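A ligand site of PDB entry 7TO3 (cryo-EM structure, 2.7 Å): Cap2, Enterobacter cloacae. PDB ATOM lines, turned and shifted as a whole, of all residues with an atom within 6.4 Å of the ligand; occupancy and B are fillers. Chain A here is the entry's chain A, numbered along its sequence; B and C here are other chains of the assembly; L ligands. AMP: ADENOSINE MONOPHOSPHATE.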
ATOM      1  N   ILE A 384     -26.063   9.366  -8.989  1.00  0.00           N
ATOM      2  CA  ILE A 384     -24.792   9.234  -8.282  1.00  0.00           C
ATOM      3  C   ILE A 384     -24.365  10.616  -7.820  1.00  0.00           C
ATOM      4  O   ILE A 384     -24.127  11.507  -8.632  1.00  0.00           O
ATOM      5  CB  ILE A 384     -23.724   8.588  -9.183  1.00  0.00           C
ATOM      6  CG1 ILE A 384     -24.279   7.317  -9.832  1.00  0.00           C
ATOM      7  CG2 ILE A 384     -22.469   8.280  -8.375  1.00  0.00           C
ATOM      8  CD1 ILE A 384     -23.341   6.686 -10.832  1.00  0.00           C
ATOM      9  N   GLY A 385     -24.256  10.792  -6.504  1.00  0.00           N
ATOM     10  CA  GLY A 385     -23.892  12.073  -5.946  1.00  0.00           C
ATOM     11  C   GLY A 385     -25.053  12.777  -5.274  1.00  0.00           C
ATOM     12  O   GLY A 385     -25.922  13.334  -5.958  1.00  0.00           O
ATOM     13  N   ALA A 386     -25.082  12.764  -3.944  1.00  0.00           N
ATOM     14  CA  ALA A 386     -26.138  13.390  -3.154  1.00  0.00           C
ATOM     15  C   ALA A 386     -25.707  14.746  -2.613  1.00  0.00           C
ATOM     16  O   ALA A 386     -26.071  15.123  -1.498  1.00  0.00           O
ATOM     17  CB  ALA A 386     -26.574  12.469  -2.022  1.00  0.00           C
ATOM     18  N   GLY A 387     -24.929  15.495  -3.385  1.00  0.00           N
ATOM     19  CA  GLY A 387     -24.414  16.771  -2.936  1.00  0.00           C
ATOM     20  C   GLY A 387     -25.367  17.926  -3.166  1.00  0.00           C
ATOM     21  O   GLY A 387     -26.524  17.886  -2.742  1.00  0.00           O
ATOM     22  N   SER A 388     -24.881  18.971  -3.839  1.00  0.00           N
ATOM     23  CA  SER A 388     -25.690  20.184  -4.034  1.00  0.00           C
ATOM     24  C   SER A 388     -26.682  20.013  -5.177  1.00  0.00           C
ATOM     25  O   SER A 388     -27.901  20.101  -4.974  1.00  0.00           O
ATOM     26  CB  SER A 388     -24.772  21.387  -4.277  1.00  0.00           C
ATOM     27  OG  SER A 388     -23.886  21.583  -3.189  1.00  0.00           O
ATOM     28  N   LEU A 389     -26.181  19.780  -6.385  1.00  0.00           N
ATOM     29  CA  LEU A 389     -27.057  19.669  -7.553  1.00  0.00           C
ATOM     30  C   LEU A 389     -27.924  18.425  -7.490  1.00  0.00           C
ATOM     31  O   LEU A 389     -29.111  18.465  -7.862  1.00  0.00           O
ATOM     32  CB  LEU A 389     -26.216  19.677  -8.832  1.00  0.00           C
ATOM     33  CG  LEU A 389     -26.878  20.132 -10.128  1.00  0.00           C
ATOM     34  CD1 LEU A 389     -27.218  21.611 -10.059  1.00  0.00           C
ATOM     35  CD2 LEU A 389     -25.991  19.836 -11.322  1.00  0.00           C
ATOM     36  N   LEU A 408     -26.807   7.138  -4.743  1.00  0.00           N
ATOM     37  CA  LEU A 408     -25.504   6.547  -4.441  1.00  0.00           C
ATOM     38  C   LEU A 408     -24.589   7.633  -3.880  1.00  0.00           C
ATOM     39  O   LEU A 408     -24.242   8.591  -4.591  1.00  0.00           O
ATOM     40  CB  LEU A 408     -24.894   5.899  -5.688  1.00  0.00           C
ATOM     41  CG  LEU A 408     -23.653   5.029  -5.482  1.00  0.00           C
ATOM     42  CD1 LEU A 408     -23.995   3.762  -4.720  1.00  0.00           C
ATOM     43  CD2 LEU A 408     -23.043   4.687  -6.825  1.00  0.00           C
ATOM     44  N   ASP A 409     -24.189   7.486  -2.620  1.00  0.00           N
ATOM     45  CA  ASP A 409     -23.262   8.405  -1.980  1.00  0.00           C
ATOM     46  C   ASP A 409     -22.707   7.760  -0.722  1.00  0.00           C
ATOM     47  O   ASP A 409     -23.357   6.902  -0.126  1.00  0.00           O
ATOM     48  CB  ASP A 409     -23.930   9.741  -1.641  1.00  0.00           C
ATOM     49  CG  ASP A 409     -22.934  10.868  -1.463  1.00  0.00           C
ATOM     50  OD1 ASP A 409     -21.721  10.578  -1.302  1.00  0.00           O
ATOM     51  OD2 ASP A 409     -23.349  12.044  -1.481  1.00  0.00           O
ATOM     52  N   ALA A 410     -21.507   8.178  -0.312  1.00  0.00           N
ATOM     53  CA  ALA A 410     -20.831   7.615   0.841  1.00  0.00           C
ATOM     54  C   ALA A 410     -20.166   8.681   1.717  1.00  0.00           C
ATOM     55  O   ALA A 410     -19.247   8.369   2.477  1.00  0.00           O
ATOM     56  CB  ALA A 410     -19.789   6.577   0.410  1.00  0.00           C
ATOM     57  N   ASP A 411     -20.614   9.932   1.616  1.00  0.00           N
ATOM     58  CA  ASP A 411     -20.061  11.023   2.401  1.00  0.00           C
ATOM     59  C   ASP A 411     -21.044  11.448   3.493  1.00  0.00           C
ATOM     60  O   ASP A 411     -22.213  11.050   3.508  1.00  0.00           O
ATOM     61  CB  ASP A 411     -19.729  12.216   1.509  1.00  0.00           C
ATOM     62  CG  ASP A 411     -18.485  11.985   0.671  1.00  0.00           C
ATOM     63  OD1 ASP A 411     -17.960  10.856   0.691  1.00  0.00           O
ATOM     64  OD2 ASP A 411     -18.031  12.939   0.003  1.00  0.00           O
ATOM     65  N   ARG A 420     -25.528  25.672   0.434  1.00  0.00           N
ATOM     66  CA  ARG A 420     -26.131  25.315  -0.847  1.00  0.00           C
ATOM     67  C   ARG A 420     -26.551  23.840  -0.786  1.00  0.00           C
ATOM     68  O   ARG A 420     -25.818  22.920  -1.141  1.00  0.00           O
ATOM     69  CB  ARG A 420     -25.188  25.608  -2.019  1.00  0.00           C
ATOM     70  CG  ARG A 420     -23.889  24.810  -2.027  1.00  0.00           C
ATOM     71  CD  ARG A 420     -22.967  25.178  -3.166  1.00  0.00           C
ATOM     72  NE  ARG A 420     -21.802  24.293  -3.154  1.00  0.00           N
ATOM     73  CZ  ARG A 420     -20.711  24.543  -2.452  1.00  0.00           C
ATOM     74  NH1 ARG A 420     -20.572  25.664  -1.770  1.00  0.00           N
ATOM     75  NH2 ARG A 420     -19.732  23.635  -2.422  1.00  0.00           N
ATOM     76  N   LYS A 432     -25.263  11.172   3.386  1.00  0.00           N
ATOM     77  CA  LYS A 432     -26.044  12.058   2.521  1.00  0.00           C
ATOM     78  C   LYS A 432     -27.173  11.316   1.838  1.00  0.00           C
ATOM     79  O   LYS A 432     -28.312  11.810   1.772  1.00  0.00           O
ATOM     80  CB  LYS A 432     -25.117  12.708   1.491  1.00  0.00           C
ATOM     81  CG  LYS A 432     -24.191  13.771   2.055  1.00  0.00           C
ATOM     82  CD  LYS A 432     -23.373  14.427   0.960  1.00  0.00           C
ATOM     83  CE  LYS A 432     -22.497  15.547   1.508  1.00  0.00           C
ATOM     84  NZ  LYS A 432     -21.735  16.242   0.432  1.00  0.00           N
ATOM     85  N   CYS A 454     -22.666   2.707  -0.370  1.00  0.00           N
ATOM     86  CA  CYS A 454     -21.353   2.383  -0.900  1.00  0.00           C
ATOM     87  C   CYS A 454     -20.933   3.401  -1.952  1.00  0.00           C
ATOM     88  O   CYS A 454     -21.717   4.250  -2.393  1.00  0.00           O
ATOM     89  CB  CYS A 454     -21.338   0.977  -1.488  1.00  0.00           C
ATOM     90  SG  CYS A 454     -21.647  -0.345  -0.292  1.00  0.00           S
ATOM     91  N   ALA A 455     -19.674   3.315  -2.351  1.00  0.00           N
ATOM     92  CA  ALA A 455     -19.101   4.192  -3.363  1.00  0.00           C
ATOM     93  C   ALA A 455     -18.931   3.431  -4.677  1.00  0.00           C
ATOM     94  O   ALA A 455     -18.566   2.254  -4.691  1.00  0.00           O
ATOM     95  CB  ALA A 455     -17.767   4.768  -2.914  1.00  0.00           C
ATOM     96  N   PHE A 456     -19.195   4.124  -5.782  1.00  0.00           N
ATOM     97  CA  PHE A 456     -19.093   3.499  -7.087  1.00  0.00           C
ATOM     98  C   PHE A 456     -17.639   3.203  -7.426  1.00  0.00           C
ATOM     99  O   PHE A 456     -16.766   4.048  -7.232  1.00  0.00           O
ATOM    100  CB  PHE A 456     -19.696   4.403  -8.168  1.00  0.00           C
ATOM    101  CG  PHE A 456     -20.158   3.670  -9.392  1.00  0.00           C
ATOM    102  CD1 PHE A 456     -21.274   2.851  -9.350  1.00  0.00           C
ATOM    103  CD2 PHE A 456     -19.480   3.801 -10.586  1.00  0.00           C
ATOM    104  CE1 PHE A 456     -21.699   2.181 -10.479  1.00  0.00           C
ATOM    105  CE2 PHE A 456     -19.895   3.130 -11.725  1.00  0.00           C
ATOM    106  CZ  PHE A 456     -21.010   2.310 -11.660  1.00  0.00           C
ATOM    107  N   PRO A 457     -17.333   1.994  -7.946  1.00  0.00           N
ATOM    108  CA  PRO A 457     -18.295   0.898  -8.079  1.00  0.00           C
ATOM    109  C   PRO A 457     -18.411   0.054  -6.809  1.00  0.00           C
ATOM    110  O   PRO A 457     -17.451  -0.036  -6.054  1.00  0.00           O
ATOM    111  CB  PRO A 457     -17.701   0.072  -9.224  1.00  0.00           C
ATOM    112  CG  PRO A 457     -16.237   0.275  -9.095  1.00  0.00           C
ATOM    113  CD  PRO A 457     -16.030   1.667  -8.547  1.00  0.00           C
ATOM    114  N   CYS A 476     -23.952  13.437 -11.109  1.00  0.00           N
ATOM    115  CA  CYS A 476     -23.914  14.802 -10.576  1.00  0.00           C
ATOM    116  C   CYS A 476     -22.801  14.897  -9.526  1.00  0.00           C
ATOM    117  O   CYS A 476     -22.976  15.437  -8.438  1.00  0.00           O
ATOM    118  CB  CYS A 476     -25.256  15.205  -9.990  1.00  0.00           C
ATOM    119  SG  CYS A 476     -26.633  15.160 -11.160  1.00  0.00           S
ATOM    120  N   THR A 477     -21.639  14.334  -9.866  1.00  0.00           N
ATOM    121  CA  THR A 477     -20.483  14.314  -8.979  1.00  0.00           C
ATOM    122  C   THR A 477     -19.401  15.305  -9.362  1.00  0.00           C
ATOM    123  O   THR A 477     -18.754  15.879  -8.487  1.00  0.00           O
ATOM    124  CB  THR A 477     -19.873  12.912  -8.919  1.00  0.00           C
ATOM    125  OG1 THR A 477     -19.448  12.531 -10.240  1.00  0.00           O
ATOM    126  CG2 THR A 477     -20.884  11.899  -8.407  1.00  0.00           C
ATOM    127  N   GLY A 478     -19.184  15.527 -10.662  1.00  0.00           N
ATOM    128  CA  GLY A 478     -18.121  16.401 -11.098  1.00  0.00           C
ATOM    129  C   GLY A 478     -16.733  15.822 -10.967  1.00  0.00           C
ATOM    130  O   GLY A 478     -15.756  16.577 -10.956  1.00  0.00           O
ATOM    131  N   ASP A 479     -16.620  14.502 -10.855  1.00  0.00           N
ATOM    132  CA  ASP A 479     -15.347  13.824 -10.683  1.00  0.00           C
ATOM    133  C   ASP A 479     -15.046  12.954 -11.899  1.00  0.00           C
ATOM    134  O   ASP A 479     -15.933  12.275 -12.422  1.00  0.00           O
ATOM    135  CB  ASP A 479     -15.357  12.963  -9.411  1.00  0.00           C
ATOM    136  CG  ASP A 479     -14.000  12.381  -9.094  1.00  0.00           C
ATOM    137  OD1 ASP A 479     -12.975  13.018  -9.417  1.00  0.00           O
ATOM    138  OD2 ASP A 479     -13.954  11.261  -8.520  1.00  0.00           O
ATOM    139  N   GLY A 481     -12.853  10.375 -12.002  1.00  0.00           N
ATOM    140  CA  GLY A 481     -12.744   8.971 -11.649  1.00  0.00           C
ATOM    141  C   GLY A 481     -14.076   8.247 -11.762  1.00  0.00           C
ATOM    142  O   GLY A 481     -14.129   7.087 -12.173  1.00  0.00           O
ATOM    143  N   VAL A 482     -15.167   8.923 -11.397  1.00  0.00           N
ATOM    144  CA  VAL A 482     -16.498   8.347 -11.573  1.00  0.00           C
ATOM    145  C   VAL A 482     -16.803   8.144 -13.045  1.00  0.00           C
ATOM    146  O   VAL A 482     -17.399   7.130 -13.437  1.00  0.00           O
ATOM    147  CB  VAL A 482     -17.558   9.236 -10.890  1.00  0.00           C
ATOM    148  CG1 VAL A 482     -18.911   8.537 -10.893  1.00  0.00           C
ATOM    149  CG2 VAL A 482     -17.126   9.579  -9.469  1.00  0.00           C
ATOM    150  N   MET A 502     -21.383  21.814 -13.217  1.00  0.00           N
ATOM    151  CA  MET A 502     -21.288  23.271 -13.251  1.00  0.00           C
ATOM    152  C   MET A 502     -19.831  23.708 -13.438  1.00  0.00           C
ATOM    153  O   MET A 502     -18.890  22.929 -13.271  1.00  0.00           O
ATOM    154  CB  MET A 502     -21.852  23.891 -11.964  1.00  0.00           C
ATOM    155  CG  MET A 502     -23.311  23.574 -11.707  1.00  0.00           C
ATOM    156  SD  MET A 502     -23.938  24.367 -10.221  1.00  0.00           S
ATOM    157  CE  MET A 502     -22.910  23.612  -8.966  1.00  0.00           C
ATOM    158  N   PHE A 553     -15.034  25.980  -3.750  1.00  0.00           N
ATOM    159  CA  PHE A 553     -15.420  26.647  -4.984  1.00  0.00           C
ATOM    160  C   PHE A 553     -16.618  27.555  -4.741  1.00  0.00           C
ATOM    161  O   PHE A 553     -17.559  27.150  -4.057  1.00  0.00           O
ATOM    162  CB  PHE A 553     -15.712  25.633  -6.099  1.00  0.00           C
ATOM    163  CG  PHE A 553     -16.980  24.850  -5.910  1.00  0.00           C
ATOM    164  CD1 PHE A 553     -16.988  23.689  -5.152  1.00  0.00           C
ATOM    165  CD2 PHE A 553     -18.162  25.265  -6.514  1.00  0.00           C
ATOM    166  CE1 PHE A 553     -18.153  22.964  -4.993  1.00  0.00           C
ATOM    167  CE2 PHE A 553     -19.326  24.541  -6.354  1.00  0.00           C
ATOM    168  CZ  PHE A 553     -19.329  23.387  -5.591  1.00  0.00           C
ATOM    169  N   PHE B 398     -17.550  21.095 -11.254  1.00  0.00           N
ATOM    170  CA  PHE B 398     -17.921  21.048  -9.853  1.00  0.00           C
ATOM    171  C   PHE B 398     -19.399  20.721  -9.729  1.00  0.00           C
ATOM    172  O   PHE B 398     -20.200  21.053 -10.603  1.00  0.00           O
ATOM    173  CB  PHE B 398     -17.627  22.383  -9.157  1.00  0.00           C
ATOM    174  CG  PHE B 398     -16.254  22.932  -9.453  1.00  0.00           C
ATOM    175  CD1 PHE B 398     -15.151  22.503  -8.724  1.00  0.00           C
ATOM    176  CD2 PHE B 398     -16.062  23.858 -10.462  1.00  0.00           C
ATOM    177  CE1 PHE B 398     -13.889  22.999  -8.990  1.00  0.00           C
ATOM    178  CE2 PHE B 398     -14.804  24.350 -10.741  1.00  0.00           C
ATOM    179  CZ  PHE B 398     -13.719  23.927 -10.002  1.00  0.00           C
ATOM    180  N   ALA B 399     -19.754  20.054  -8.635  1.00  0.00           N
ATOM    181  CA  ALA B 399     -21.143  19.679  -8.380  1.00  0.00           C
ATOM    182  C   ALA B 399     -21.487  19.817  -6.892  1.00  0.00           C
ATOM    183  O   ALA B 399     -22.587  20.204  -6.492  1.00  0.00           O
ATOM    184  CB  ALA B 399     -21.406  18.260  -8.850  1.00  0.00           C
ATOM    185  N   GLU C  69     -10.159   0.204  -5.641  1.00  0.00           N
ATOM    186  CA  GLU C  69     -11.249  -0.231  -6.504  1.00  0.00           C
ATOM    187  C   GLU C  69     -10.808  -0.120  -7.950  1.00  0.00           C
ATOM    188  O   GLU C  69     -10.748  -1.142  -8.655  1.00  0.00           O
ATOM    189  CB  GLU C  69     -12.519   0.589  -6.217  1.00  0.00           C
ATOM    190  CG  GLU C  69     -13.245   0.228  -4.932  1.00  0.00           C
ATOM    191  CD  GLU C  69     -14.477   1.084  -4.722  1.00  0.00           C
ATOM    192  OE1 GLU C  69     -14.551   2.180  -5.314  1.00  0.00           O
ATOM    193  OE2 GLU C  69     -15.373   0.664  -3.957  1.00  0.00           O
HETATM  194  P   AMP L   1     -20.195  18.409  -4.660  1.00  0.00           P
HETATM  195  O1P AMP L   1     -21.009  18.427  -3.385  1.00  0.00           O
HETATM  196  O2P AMP L   1     -18.713  18.205  -4.446  1.00  0.00           O
HETATM  197  O3P AMP L   1     -20.526  19.496  -5.650  1.00  0.00           O
HETATM  198  O5' AMP L   1     -20.655  17.077  -5.399  1.00  0.00           O
HETATM  199  C5' AMP L   1     -19.977  15.838  -5.176  1.00  0.00           C
HETATM  200  C4' AMP L   1     -20.916  14.771  -4.675  1.00  0.00           C
HETATM  201  O4' AMP L   1     -20.647  13.533  -5.389  1.00  0.00           O
HETATM  202  C3' AMP L   1     -20.799  14.450  -3.186  1.00  0.00           C
HETATM  203  O3' AMP L   1     -22.089  14.136  -2.664  1.00  0.00           O
HETATM  204  C2' AMP L   1     -19.934  13.188  -3.186  1.00  0.00           C
HETATM  205  O2' AMP L   1     -20.099  12.362  -2.042  1.00  0.00           O
HETATM  206  C1' AMP L   1     -20.389  12.493  -4.459  1.00  0.00           C
HETATM  207  N9  AMP L   1     -19.385  11.593  -5.045  1.00  0.00           N
HETATM  208  C8  AMP L   1     -18.248  11.976  -5.643  1.00  0.00           C
HETATM  209  N7  AMP L   1     -17.534  10.903  -6.079  1.00  0.00           N
HETATM  210  C5  AMP L   1     -18.232   9.799  -5.753  1.00  0.00           C
HETATM  211  C6  AMP L   1     -18.055   8.339  -5.914  1.00  0.00           C
HETATM  212  N6  AMP L   1     -16.971   7.826  -6.528  1.00  0.00           N
HETATM  213  N1  AMP L   1     -19.025   7.532  -5.426  1.00  0.00           N
HETATM  214  C2  AMP L   1     -20.121   8.025  -4.812  1.00  0.00           C
HETATM  215  N3  AMP L   1     -20.347   9.343  -4.630  1.00  0.00           N
HETATM  216  C4  AMP L   1     -19.455  10.263  -5.066  1.00  0.00           C
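N of Phe 456 lies within hydrogen-bond range of N1 of the ligand (3.4 Å).
The side-chain carboxylate (OD2) of Asp 411 lies within hydrogen-bond range of an oxygen (O2') of the ligand.
N of Ala 399 of chain B sits close to O3P of the ligand (3.1 Å).
OD1 of Asp 409 lies within hydrogen-bond range of O2' of the ligand, at 2.5 Å.
O3' of the ligand lies within hydrogen-bond range of N of Gly 387.
The side-chain hydroxyl (OG) of Ser 388 sits at hydrogen-bond distance from the backbone carbonyl oxygen (O) of Arg 420.
The backbone NH (N) of Asp 411 lies within hydrogen-bond range of the side-chain carboxylate (OD1) of Asp 409.
The side-chain carboxylate of Asp 409 lies within hydrogen-bond range of the backbone NH of Ala 386 (3.1 Å).
O of Leu 408 lies within hydrogen-bond range of N of Gly 385, at 2.9 Å.
The backbone carbonyl oxygen (O) of Asp 411 lies within hydrogen-bond range of the backbone NH (N) of Lys 432 (3.1 Å).
Merely in contact with the ligand: Val 482, Thr 477, Ala 386, Gly 385, Lys 432, Ala 455, Ser 388 and Leu 408.
13 residues have an atom within 4 Å of the ligand: Gly 385, Ala 386, Gly 387, Ser 388, Leu 408, Asp 409, Asp 411, Lys 432, Ala 455, Phe 456, Thr 477, Val 482 and Ala 399 of chain B.
Along chain A the residues within 4 Å of the ligand span positions 385 to 482.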
